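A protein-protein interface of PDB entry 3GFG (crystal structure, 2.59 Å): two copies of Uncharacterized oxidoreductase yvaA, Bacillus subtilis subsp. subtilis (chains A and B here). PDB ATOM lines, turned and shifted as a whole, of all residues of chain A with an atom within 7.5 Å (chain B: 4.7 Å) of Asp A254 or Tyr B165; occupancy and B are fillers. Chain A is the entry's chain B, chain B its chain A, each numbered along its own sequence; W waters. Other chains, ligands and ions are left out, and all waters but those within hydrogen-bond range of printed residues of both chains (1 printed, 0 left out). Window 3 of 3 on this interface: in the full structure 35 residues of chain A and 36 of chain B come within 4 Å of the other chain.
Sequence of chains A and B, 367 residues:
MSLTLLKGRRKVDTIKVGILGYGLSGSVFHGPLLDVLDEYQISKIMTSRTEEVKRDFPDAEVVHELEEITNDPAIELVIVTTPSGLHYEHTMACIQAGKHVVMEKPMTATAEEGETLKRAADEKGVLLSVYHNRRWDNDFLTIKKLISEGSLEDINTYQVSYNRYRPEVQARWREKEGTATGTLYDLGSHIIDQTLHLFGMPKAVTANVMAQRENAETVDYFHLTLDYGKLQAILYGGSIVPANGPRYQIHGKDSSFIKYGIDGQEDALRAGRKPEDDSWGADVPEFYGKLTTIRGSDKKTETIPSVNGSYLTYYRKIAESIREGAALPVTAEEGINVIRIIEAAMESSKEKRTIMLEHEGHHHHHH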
ATOM      1  N   GLY A 150      29.492 -11.125  -3.762  1.00  0.00           N
ATOM      2  CA  GLY A 150      28.074 -11.386  -3.845  1.00  0.00           C
ATOM      3  C   GLY A 150      27.655 -12.830  -3.669  1.00  0.00           C
ATOM      4  O   GLY A 150      26.542 -13.182  -4.040  1.00  0.00           O
ATOM      5  N   SER A 151      28.518 -13.662  -3.087  1.00  0.00           N
ATOM      6  CA  SER A 151      28.191 -15.086  -2.874  1.00  0.00           C
ATOM      7  C   SER A 151      27.539 -15.367  -1.541  1.00  0.00           C
ATOM      8  O   SER A 151      27.127 -16.483  -1.307  1.00  0.00           O
ATOM      9  CB  SER A 151      29.425 -15.972  -3.002  1.00  0.00           C
ATOM     10  OG  SER A 151      30.043 -15.768  -4.257  1.00  0.00           O
ATOM     11  N   LEU A 152      27.475 -14.367  -0.663  1.00  0.00           N
ATOM     12  CA  LEU A 152      26.788 -14.510   0.609  1.00  0.00           C
ATOM     13  C   LEU A 152      25.917 -13.298   0.872  1.00  0.00           C
ATOM     14  O   LEU A 152      26.183 -12.490   1.752  1.00  0.00           O
ATOM     15  CB  LEU A 152      27.776 -14.678   1.748  1.00  0.00           C
ATOM     16  CG  LEU A 152      28.333 -16.053   2.042  1.00  0.00           C
ATOM     17  CD1 LEU A 152      29.415 -15.872   3.095  1.00  0.00           C
ATOM     18  CD2 LEU A 152      27.227 -17.029   2.507  1.00  0.00           C
ATOM     19  N   GLU A 153      24.849 -13.192   0.103  1.00  0.00           N
ATOM     20  CA  GLU A 153      24.019 -12.009   0.113  1.00  0.00           C
ATOM     21  C   GLU A 153      23.028 -12.123   1.237  1.00  0.00           C
ATOM     22  O   GLU A 153      22.522 -13.201   1.483  1.00  0.00           O
ATOM     23  CB  GLU A 153      23.293 -11.895  -1.221  1.00  0.00           C
ATOM     24  CG  GLU A 153      24.152 -11.421  -2.327  1.00  0.00           C
ATOM     25  CD  GLU A 153      24.073  -9.919  -2.482  1.00  0.00           C
ATOM     26  OE1 GLU A 153      23.187  -9.450  -3.250  1.00  0.00           O
ATOM     27  OE2 GLU A 153      24.895  -9.210  -1.834  1.00  0.00           O
ATOM     28  N   ASP A 154      22.763 -11.006   1.906  1.00  0.00           N
ATOM     29  CA  ASP A 154      21.711 -10.899   2.924  1.00  0.00           C
ATOM     30  C   ASP A 154      21.744 -12.042   3.973  1.00  0.00           C
ATOM     31  O   ASP A 154      20.828 -12.876   4.080  1.00  0.00           O
ATOM     32  CB  ASP A 154      20.334 -10.732   2.248  1.00  0.00           C
ATOM     33  CG  ASP A 154      19.229 -10.283   3.225  1.00  0.00           C
ATOM     34  OD1 ASP A 154      19.370 -10.443   4.476  1.00  0.00           O
ATOM     35  OD2 ASP A 154      18.195  -9.767   2.730  1.00  0.00           O
ATOM     36  N   ASN A 156      21.369 -14.061   7.201  1.00  0.00           N
ATOM     37  CA  ASN A 156      20.326 -14.073   8.201  1.00  0.00           C
ATOM     38  C   ASN A 156      20.794 -14.778   9.444  1.00  0.00           C
ATOM     39  O   ASN A 156      20.304 -14.506  10.529  1.00  0.00           O
ATOM     40  CB  ASN A 156      19.045 -14.713   7.668  1.00  0.00           C
ATOM     41  CG  ASN A 156      19.251 -16.140   7.188  1.00  0.00           C
ATOM     42  OD1 ASN A 156      19.446 -17.064   7.987  1.00  0.00           O
ATOM     43  ND2 ASN A 156      19.196 -16.333   5.873  1.00  0.00           N
ATOM     44  N   HIS A 251      24.383 -18.510   6.927  1.00  0.00           N
ATOM     45  CA  HIS A 251      23.246 -18.634   6.008  1.00  0.00           C
ATOM     46  C   HIS A 251      22.755 -17.293   5.495  1.00  0.00           C
ATOM     47  O   HIS A 251      22.512 -16.356   6.281  1.00  0.00           O
ATOM     48  CB  HIS A 251      22.093 -19.428   6.649  1.00  0.00           C
ATOM     49  CG  HIS A 251      22.547 -20.682   7.316  1.00  0.00           C
ATOM     50  ND1 HIS A 251      23.240 -21.669   6.643  1.00  0.00           N
ATOM     51  CD2 HIS A 251      22.474 -21.080   8.606  1.00  0.00           C
ATOM     52  CE1 HIS A 251      23.566 -22.624   7.494  1.00  0.00           C
ATOM     53  NE2 HIS A 251      23.107 -22.295   8.689  1.00  0.00           N
ATOM     54  N   GLY A 252      22.643 -17.215   4.171  1.00  0.00           N
ATOM     55  CA  GLY A 252      22.134 -16.028   3.460  1.00  0.00           C
ATOM     56  C   GLY A 252      20.845 -16.424   2.790  1.00  0.00           C
ATOM     57  O   GLY A 252      20.378 -17.547   2.950  1.00  0.00           O
ATOM     58  N   LYS A 253      20.264 -15.514   2.027  1.00  0.00           N
ATOM     59  CA  LYS A 253      18.976 -15.781   1.380  1.00  0.00           C
ATOM     60  C   LYS A 253      19.033 -16.845   0.280  1.00  0.00           C
ATOM     61  O   LYS A 253      18.025 -17.482  -0.022  1.00  0.00           O
ATOM     62  CB  LYS A 253      18.350 -14.480   0.853  1.00  0.00           C
ATOM     63  CG  LYS A 253      18.936 -13.928  -0.423  1.00  0.00           C
ATOM     64  CD  LYS A 253      18.086 -12.759  -0.917  1.00  0.00           C
ATOM     65  CE  LYS A 253      18.937 -11.698  -1.605  1.00  0.00           C
ATOM     66  NZ  LYS A 253      19.383 -12.222  -2.910  1.00  0.00           N
ATOM     67  N   ASP A 254      20.219 -17.042  -0.293  1.00  0.00           N
ATOM     68  CA  ASP A 254      20.395 -17.891  -1.475  1.00  0.00           C
ATOM     69  C   ASP A 254      21.423 -18.969  -1.256  1.00  0.00           C
ATOM     70  O   ASP A 254      21.492 -19.922  -2.018  1.00  0.00           O
ATOM     71  CB  ASP A 254      20.913 -17.044  -2.644  1.00  0.00           C
ATOM     72  CG  ASP A 254      19.833 -16.254  -3.317  1.00  0.00           C
ATOM     73  OD1 ASP A 254      20.173 -15.499  -4.244  1.00  0.00           O
ATOM     74  OD2 ASP A 254      18.640 -16.386  -2.938  1.00  0.00           O
ATOM     75  N   SER A 255      22.257 -18.786  -0.246  1.00  0.00           N
ATOM     76  CA  SER A 255      23.465 -19.577  -0.122  1.00  0.00           C
ATOM     77  C   SER A 255      23.886 -19.784   1.336  1.00  0.00           C
ATOM     78  O   SER A 255      23.500 -19.005   2.222  1.00  0.00           O
ATOM     79  CB  SER A 255      24.590 -18.905  -0.912  1.00  0.00           C
ATOM     80  OG  SER A 255      24.862 -17.646  -0.338  1.00  0.00           O
ATOM     81  N   SER A 256      24.644 -20.861   1.565  1.00  0.00           N
ATOM     82  CA  SER A 256      25.267 -21.140   2.853  1.00  0.00           C
ATOM     83  C   SER A 256      26.764 -21.357   2.698  1.00  0.00           C
ATOM     84  O   SER A 256      27.220 -21.825   1.667  1.00  0.00           O
ATOM     85  CB  SER A 256      24.640 -22.387   3.483  1.00  0.00           C
ATOM     86  OG  SER A 256      23.337 -22.127   4.004  1.00  0.00           O
ATOM     87  N   THR A 292      27.140 -23.505  -0.673  1.00  0.00           N
ATOM     88  CA  THR A 292      25.918 -24.049  -1.263  1.00  0.00           C
ATOM     89  C   THR A 292      25.056 -22.906  -1.790  1.00  0.00           C
ATOM     90  O   THR A 292      24.712 -22.019  -1.035  1.00  0.00           O
ATOM     91  CB  THR A 292      25.138 -24.861  -0.219  1.00  0.00           C
ATOM     92  OG1 THR A 292      25.916 -26.007   0.177  1.00  0.00           O
ATOM     93  CG2 THR A 292      23.778 -25.309  -0.750  1.00  0.00           C
ATOM     94  N   THR A 293      24.739 -22.920  -3.081  1.00  0.00           N
ATOM     95  CA  THR A 293      23.974 -21.853  -3.707  1.00  0.00           C
ATOM     96  C   THR A 293      22.726 -22.474  -4.271  1.00  0.00           C
ATOM     97  O   THR A 293      22.786 -23.548  -4.868  1.00  0.00           O
ATOM     98  CB  THR A 293      24.742 -21.184  -4.886  1.00  0.00           C
ATOM     99  OG1 THR A 293      26.023 -20.752  -4.436  1.00  0.00           O
ATOM    100  CG2 THR A 293      23.980 -19.968  -5.442  1.00  0.00           C
ATOM    101  N   ILE A 294      21.597 -21.796  -4.092  1.00  0.00           N
ATOM    102  CA  ILE A 294      20.324 -22.285  -4.596  1.00  0.00           C
ATOM    103  C   ILE A 294      19.760 -21.262  -5.560  1.00  0.00           C
ATOM    104  O   ILE A 294      19.586 -20.102  -5.200  1.00  0.00           O
ATOM    105  CB  ILE A 294      19.345 -22.582  -3.449  1.00  0.00           C
ATOM    106  CG1 ILE A 294      19.944 -23.682  -2.556  1.00  0.00           C
ATOM    107  CG2 ILE A 294      17.984 -22.972  -4.011  1.00  0.00           C
ATOM    108  CD1 ILE A 294      19.044 -24.240  -1.487  1.00  0.00           C
ATOM    109  N   ARG A 295      19.519 -21.695  -6.797  1.00  0.00           N
ATOM    110  CA  ARG A 295      18.961 -20.836  -7.842  1.00  0.00           C
ATOM    111  C   ARG A 295      17.690 -21.482  -8.386  1.00  0.00           C
ATOM    112  O   ARG A 295      17.741 -22.379  -9.231  1.00  0.00           O
ATOM    113  CB  ARG A 295      19.984 -20.556  -8.955  1.00  0.00           C
ATOM    114  N   GLY A 296      16.557 -21.017  -7.865  1.00  0.00           N
ATOM    115  CA  GLY A 296      15.267 -21.611  -8.129  1.00  0.00           C
ATOM    116  C   GLY A 296      15.260 -23.024  -7.610  1.00  0.00           C
ATOM    117  O   GLY A 296      15.410 -23.251  -6.414  1.00  0.00           O
ATOM    118  N   ASP A 298      17.540 -25.259  -8.633  1.00  0.00           N
ATOM    119  CA  ASP A 298      18.923 -25.772  -8.757  1.00  0.00           C
ATOM    120  C   ASP A 298      19.775 -25.531  -7.504  1.00  0.00           C
ATOM    121  O   ASP A 298      20.024 -24.385  -7.112  1.00  0.00           O
ATOM    122  CB  ASP A 298      19.643 -25.172  -9.984  1.00  0.00           C
ATOM    123  CG  ASP A 298      19.243 -25.837 -11.312  1.00  0.00           C
ATOM    124  OD1 ASP A 298      18.277 -26.654 -11.338  1.00  0.00           O
ATOM    125  OD2 ASP A 298      19.901 -25.526 -12.345  1.00  0.00           O
ATOM    126  N   LYS A 299      20.233 -26.620  -6.895  1.00  0.00           N
ATOM    127  CA  LYS A 299      21.068 -26.568  -5.701  1.00  0.00           C
ATOM    128  C   LYS A 299      22.455 -27.077  -6.066  1.00  0.00           C
ATOM    129  O   LYS A 299      22.600 -28.226  -6.487  1.00  0.00           O
ATOM    130  CB  LYS A 299      20.439 -27.413  -4.566  1.00  0.00           C
ATOM    131  CG  LYS A 299      21.394 -27.829  -3.427  1.00  0.00           C
ATOM    132  CD  LYS A 299      20.753 -27.694  -2.045  1.00  0.00           C
ATOM    133  CE  LYS A 299      21.351 -28.674  -1.048  1.00  0.00           C
ATOM    134  NZ  LYS A 299      20.915 -28.426   0.373  1.00  0.00           N
ATOM    135  N   LYS A 300      23.465 -26.216  -5.939  1.00  0.00           N
ATOM    136  CA  LYS A 300      24.845 -26.652  -6.137  1.00  0.00           C
ATOM    137  C   LYS A 300      25.722 -26.377  -4.926  1.00  0.00           C
ATOM    138  O   LYS A 300      25.406 -25.557  -4.061  1.00  0.00           O
ATOM    139  CB  LYS A 300      25.464 -26.088  -7.434  1.00  0.00           C
ATOM    140  CG  LYS A 300      26.087 -24.676  -7.327  1.00  0.00           C
ATOM    141  CD  LYS A 300      26.660 -24.205  -8.685  1.00  0.00           C
ATOM    142  CE  LYS A 300      26.262 -22.754  -9.015  1.00  0.00           C
ATOM    143  NZ  LYS A 300      26.948 -21.744  -8.170  1.00  0.00           N
ATOM    144  N   ARG B 164      15.503 -25.756   7.578  1.00  0.00           N
ATOM    145  CA  ARG B 164      14.926 -26.035   6.265  1.00  0.00           C
ATOM    146  C   ARG B 164      15.166 -24.817   5.343  1.00  0.00           C
ATOM    147  O   ARG B 164      15.553 -23.729   5.821  1.00  0.00           O
ATOM    148  CB  ARG B 164      13.442 -26.411   6.398  1.00  0.00           C
ATOM    149  CG  ARG B 164      12.499 -25.222   6.541  1.00  0.00           C
ATOM    150  CD  ARG B 164      11.516 -25.390   7.697  1.00  0.00           C
ATOM    151  NE  ARG B 164      10.669 -24.204   7.815  1.00  0.00           N
ATOM    152  CZ  ARG B 164       9.356 -24.204   7.568  1.00  0.00           C
ATOM    153  NH1 ARG B 164       8.635 -23.077   7.678  1.00  0.00           N
ATOM    154  NH2 ARG B 164       8.759 -25.343   7.219  1.00  0.00           N
ATOM    155  N   TYR B 165      15.002 -25.015   4.034  1.00  0.00           N
ATOM    156  CA  TYR B 165      14.989 -23.900   3.110  1.00  0.00           C
ATOM    157  C   TYR B 165      13.602 -23.672   2.524  1.00  0.00           C
ATOM    158  O   TYR B 165      13.222 -24.290   1.526  1.00  0.00           O
ATOM    159  CB  TYR B 165      16.048 -24.070   2.011  1.00  0.00           C
ATOM    160  CG  TYR B 165      16.267 -22.843   1.119  1.00  0.00           C
ATOM    161  CD1 TYR B 165      16.854 -21.675   1.624  1.00  0.00           C
ATOM    162  CD2 TYR B 165      15.892 -22.850  -0.213  1.00  0.00           C
ATOM    163  CE1 TYR B 165      17.064 -20.545   0.821  1.00  0.00           C
ATOM    164  CE2 TYR B 165      16.110 -21.725  -1.046  1.00  0.00           C
ATOM    165  CZ  TYR B 165      16.699 -20.583  -0.519  1.00  0.00           C
ATOM    166  OH  TYR B 165      16.894 -19.460  -1.319  1.00  0.00           O
ATOM    167  N   ARG B 166      12.844 -22.781   3.151  1.00  0.00           N
ATOM    168  CA  ARG B 166      11.601 -22.272   2.553  1.00  0.00           C
ATOM    169  C   ARG B 166      11.552 -20.734   2.611  1.00  0.00           C
ATOM    170  O   ARG B 166      10.865 -20.180   3.449  1.00  0.00           O
ATOM    171  CB  ARG B 166      10.346 -22.860   3.236  1.00  0.00           C
ATOM    172  CG  ARG B 166      10.333 -24.358   3.539  1.00  0.00           C
ATOM    173  CD  ARG B 166       8.941 -24.990   3.220  1.00  0.00           C
ATOM    174  NE  ARG B 166       8.735 -26.323   3.820  1.00  0.00           N
ATOM    175  CZ  ARG B 166       9.544 -27.375   3.651  1.00  0.00           C
ATOM    176  NH1 ARG B 166      10.641 -27.276   2.901  1.00  0.00           N
ATOM    177  NH2 ARG B 166       9.267 -28.529   4.249  1.00  0.00           N
ATOM    178  N   PRO B 167      12.287 -20.036   1.730  1.00  0.00           N
ATOM    179  CA  PRO B 167      12.290 -18.573   1.822  1.00  0.00           C
ATOM    180  C   PRO B 167      10.922 -17.877   1.582  1.00  0.00           C
ATOM    181  O   PRO B 167      10.746 -16.705   1.963  1.00  0.00           O
ATOM    182  CB  PRO B 167      13.299 -18.163   0.744  1.00  0.00           C
ATOM    183  CG  PRO B 167      13.348 -19.301  -0.198  1.00  0.00           C
ATOM    184  CD  PRO B 167      13.188 -20.511   0.667  1.00  0.00           C
ATOM    185  N   SER B 239      14.417 -21.116   8.758  1.00  0.00           N
ATOM    186  CA  SER B 239      13.724 -21.454   7.515  1.00  0.00           C
ATOM    187  C   SER B 239      14.383 -20.898   6.249  1.00  0.00           C
ATOM    188  O   SER B 239      13.901 -21.156   5.143  1.00  0.00           O
ATOM    189  CB  SER B 239      12.292 -20.935   7.588  1.00  0.00           C
ATOM    190  OG  SER B 239      11.549 -21.681   8.531  1.00  0.00           O
ATOM    191  N   ILE B 240      15.442 -20.102   6.397  1.00  0.00           N
ATOM    192  CA  ILE B 240      16.212 -19.666   5.245  1.00  0.00           C
ATOM    193  C   ILE B 240      17.625 -20.241   5.344  1.00  0.00           C
ATOM    194  O   ILE B 240      18.603 -19.492   5.458  1.00  0.00           O
ATOM    195  CB  ILE B 240      16.295 -18.113   5.116  1.00  0.00           C
ATOM    196  CG1 ILE B 240      15.026 -17.445   5.653  1.00  0.00           C
ATOM    197  CG2 ILE B 240      16.575 -17.716   3.679  1.00  0.00           C
ATOM    198  CD1 ILE B 240      15.070 -15.932   5.668  1.00  0.00           C
ATOM    199  N   VAL B 241      17.725 -21.571   5.295  1.00  0.00           N
ATOM    200  CA  VAL B 241      19.009 -22.277   5.407  1.00  0.00           C
ATOM    201  C   VAL B 241      19.259 -23.166   4.169  1.00  0.00           C
ATOM    202  O   VAL B 241      18.808 -24.316   4.111  1.00  0.00           O
ATOM    203  CB  VAL B 241      19.075 -23.121   6.711  1.00  0.00           C
ATOM    204  CG1 VAL B 241      20.413 -23.762   6.879  1.00  0.00           C
ATOM    205  CG2 VAL B 241      18.774 -22.259   7.958  1.00  0.00           C
ATOM    206  N   PRO B 242      19.970 -22.628   3.163  1.00  0.00           N
ATOM    207  CA  PRO B 242      20.401 -23.410   1.986  1.00  0.00           C
ATOM    208  C   PRO B 242      21.082 -24.736   2.310  1.00  0.00           C
ATOM    209  O   PRO B 242      20.737 -25.734   1.694  1.00  0.00           O
ATOM    210  CB  PRO B 242      21.351 -22.467   1.279  1.00  0.00           C
ATOM    211  CG  PRO B 242      20.781 -21.139   1.609  1.00  0.00           C
ATOM    212  CD  PRO B 242      20.336 -21.212   3.028  1.00  0.00           C
HETATM  213  O   HOH W   1      17.281 -19.022   8.639  1.00  0.00           O
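The side-chain hydroxyl of Tyr B165 lies within hydrogen-bond range of the backbone carbonyl oxygen of Lys A253. The side-chain amide nitrogen (ND2) of Asn A156 sits at hydrogen-bond distance from the backbone carbonyl oxygen (O) of Ile B240 (3.2 Å). O of Pro B242 is in hydrogen-bond range of NZ of Lys A299, at 3.0 Å.
Water W1 bridges OD1 of Asn A156 (3.0 Å) and N of Ile B240 (3.1 Å).
No position is printed for both chains.
The backbone carbonyl oxygen (O) of Ser A151 is in hydrogen-bond range of the side-chain hydroxyl (OG) of Ser A255, 2.7 Å away. O of Asp A154 lies within hydrogen-bond range of N of Lys A253, 3.4 Å away. The backbone NH (N) of Asn A156 is in hydrogen-bond range of the backbone carbonyl oxygen (O) of His A251. A ring nitrogen (ND1) of His A251 is in hydrogen-bond range of the side-chain hydroxyl of Ser A256 (2.7 Å). The side-chain amino group (NZ) of Lys A253 is in salt-bridge range of the side-chain carboxylate (OD1) of Asp A254 (3.6 Å). The backbone NH of Ser A256 lies within hydrogen-bond range of the backbone carbonyl oxygen of Thr A292, at 2.8 Å.
Asp A254 touches just these residues of chain B: Tyr B165 (3.8 Å) and Pro B242 (3.7 Å). Tyr B165 touches just these residues of chain A: Lys A253, Asp A254 and Ile A294. Of the printed residues of chain B, His A251 touches Ile B240 and Val B241. Printed residues of chain B within 4 Å of Ser A256: Pro B242. Printed residues of chain B within 4 Å of Ser A255: Pro B242. Of the printed residues of chain B, Lys A299 touches Pro B242 (3.0 Å). Thr A293 touches none of the printed residues of chain B. Arg A295 touches none of the printed residues of chain B. The nearest printed residue of chain B that does not touch Asp A254 is Ile B240 (5.4 Å). The nearest printed residue of chain B that does not touch Lys A299 is Val B241 (5.9 Å).
Hydrophobic or aromatic side chains of chain B that line the printed part of chain A: Tyr B165, Ile B240, Val B241 and Pro B242. Of the 20 printed residues of chain A, 10 touch a printed residue of chain B.
Among the printed residues, pairs that only touch across the chains: His A251 with Ile B240 (3.7 Å), His A251 with Val B241 (3.4 Å), Gly A252 with Ile B240 (3.6 Å), Gly A252 with Pro B242 (3.7 Å), Lys A253 with Ile B240 (3.8 Å), Asp A254 with Tyr B165 (3.8 Å), Asp A254 with Pro B242 (3.7 Å), Ser A255 with Pro B242 (3.3 Å), Ser A256 with Pro B242 (3.3 Å), Thr A292 with Pro B242 (3.9 Å), Ile A294 with Tyr B165 (3.7 Å) and Ile A294 with Pro B242 (3.8 Å).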
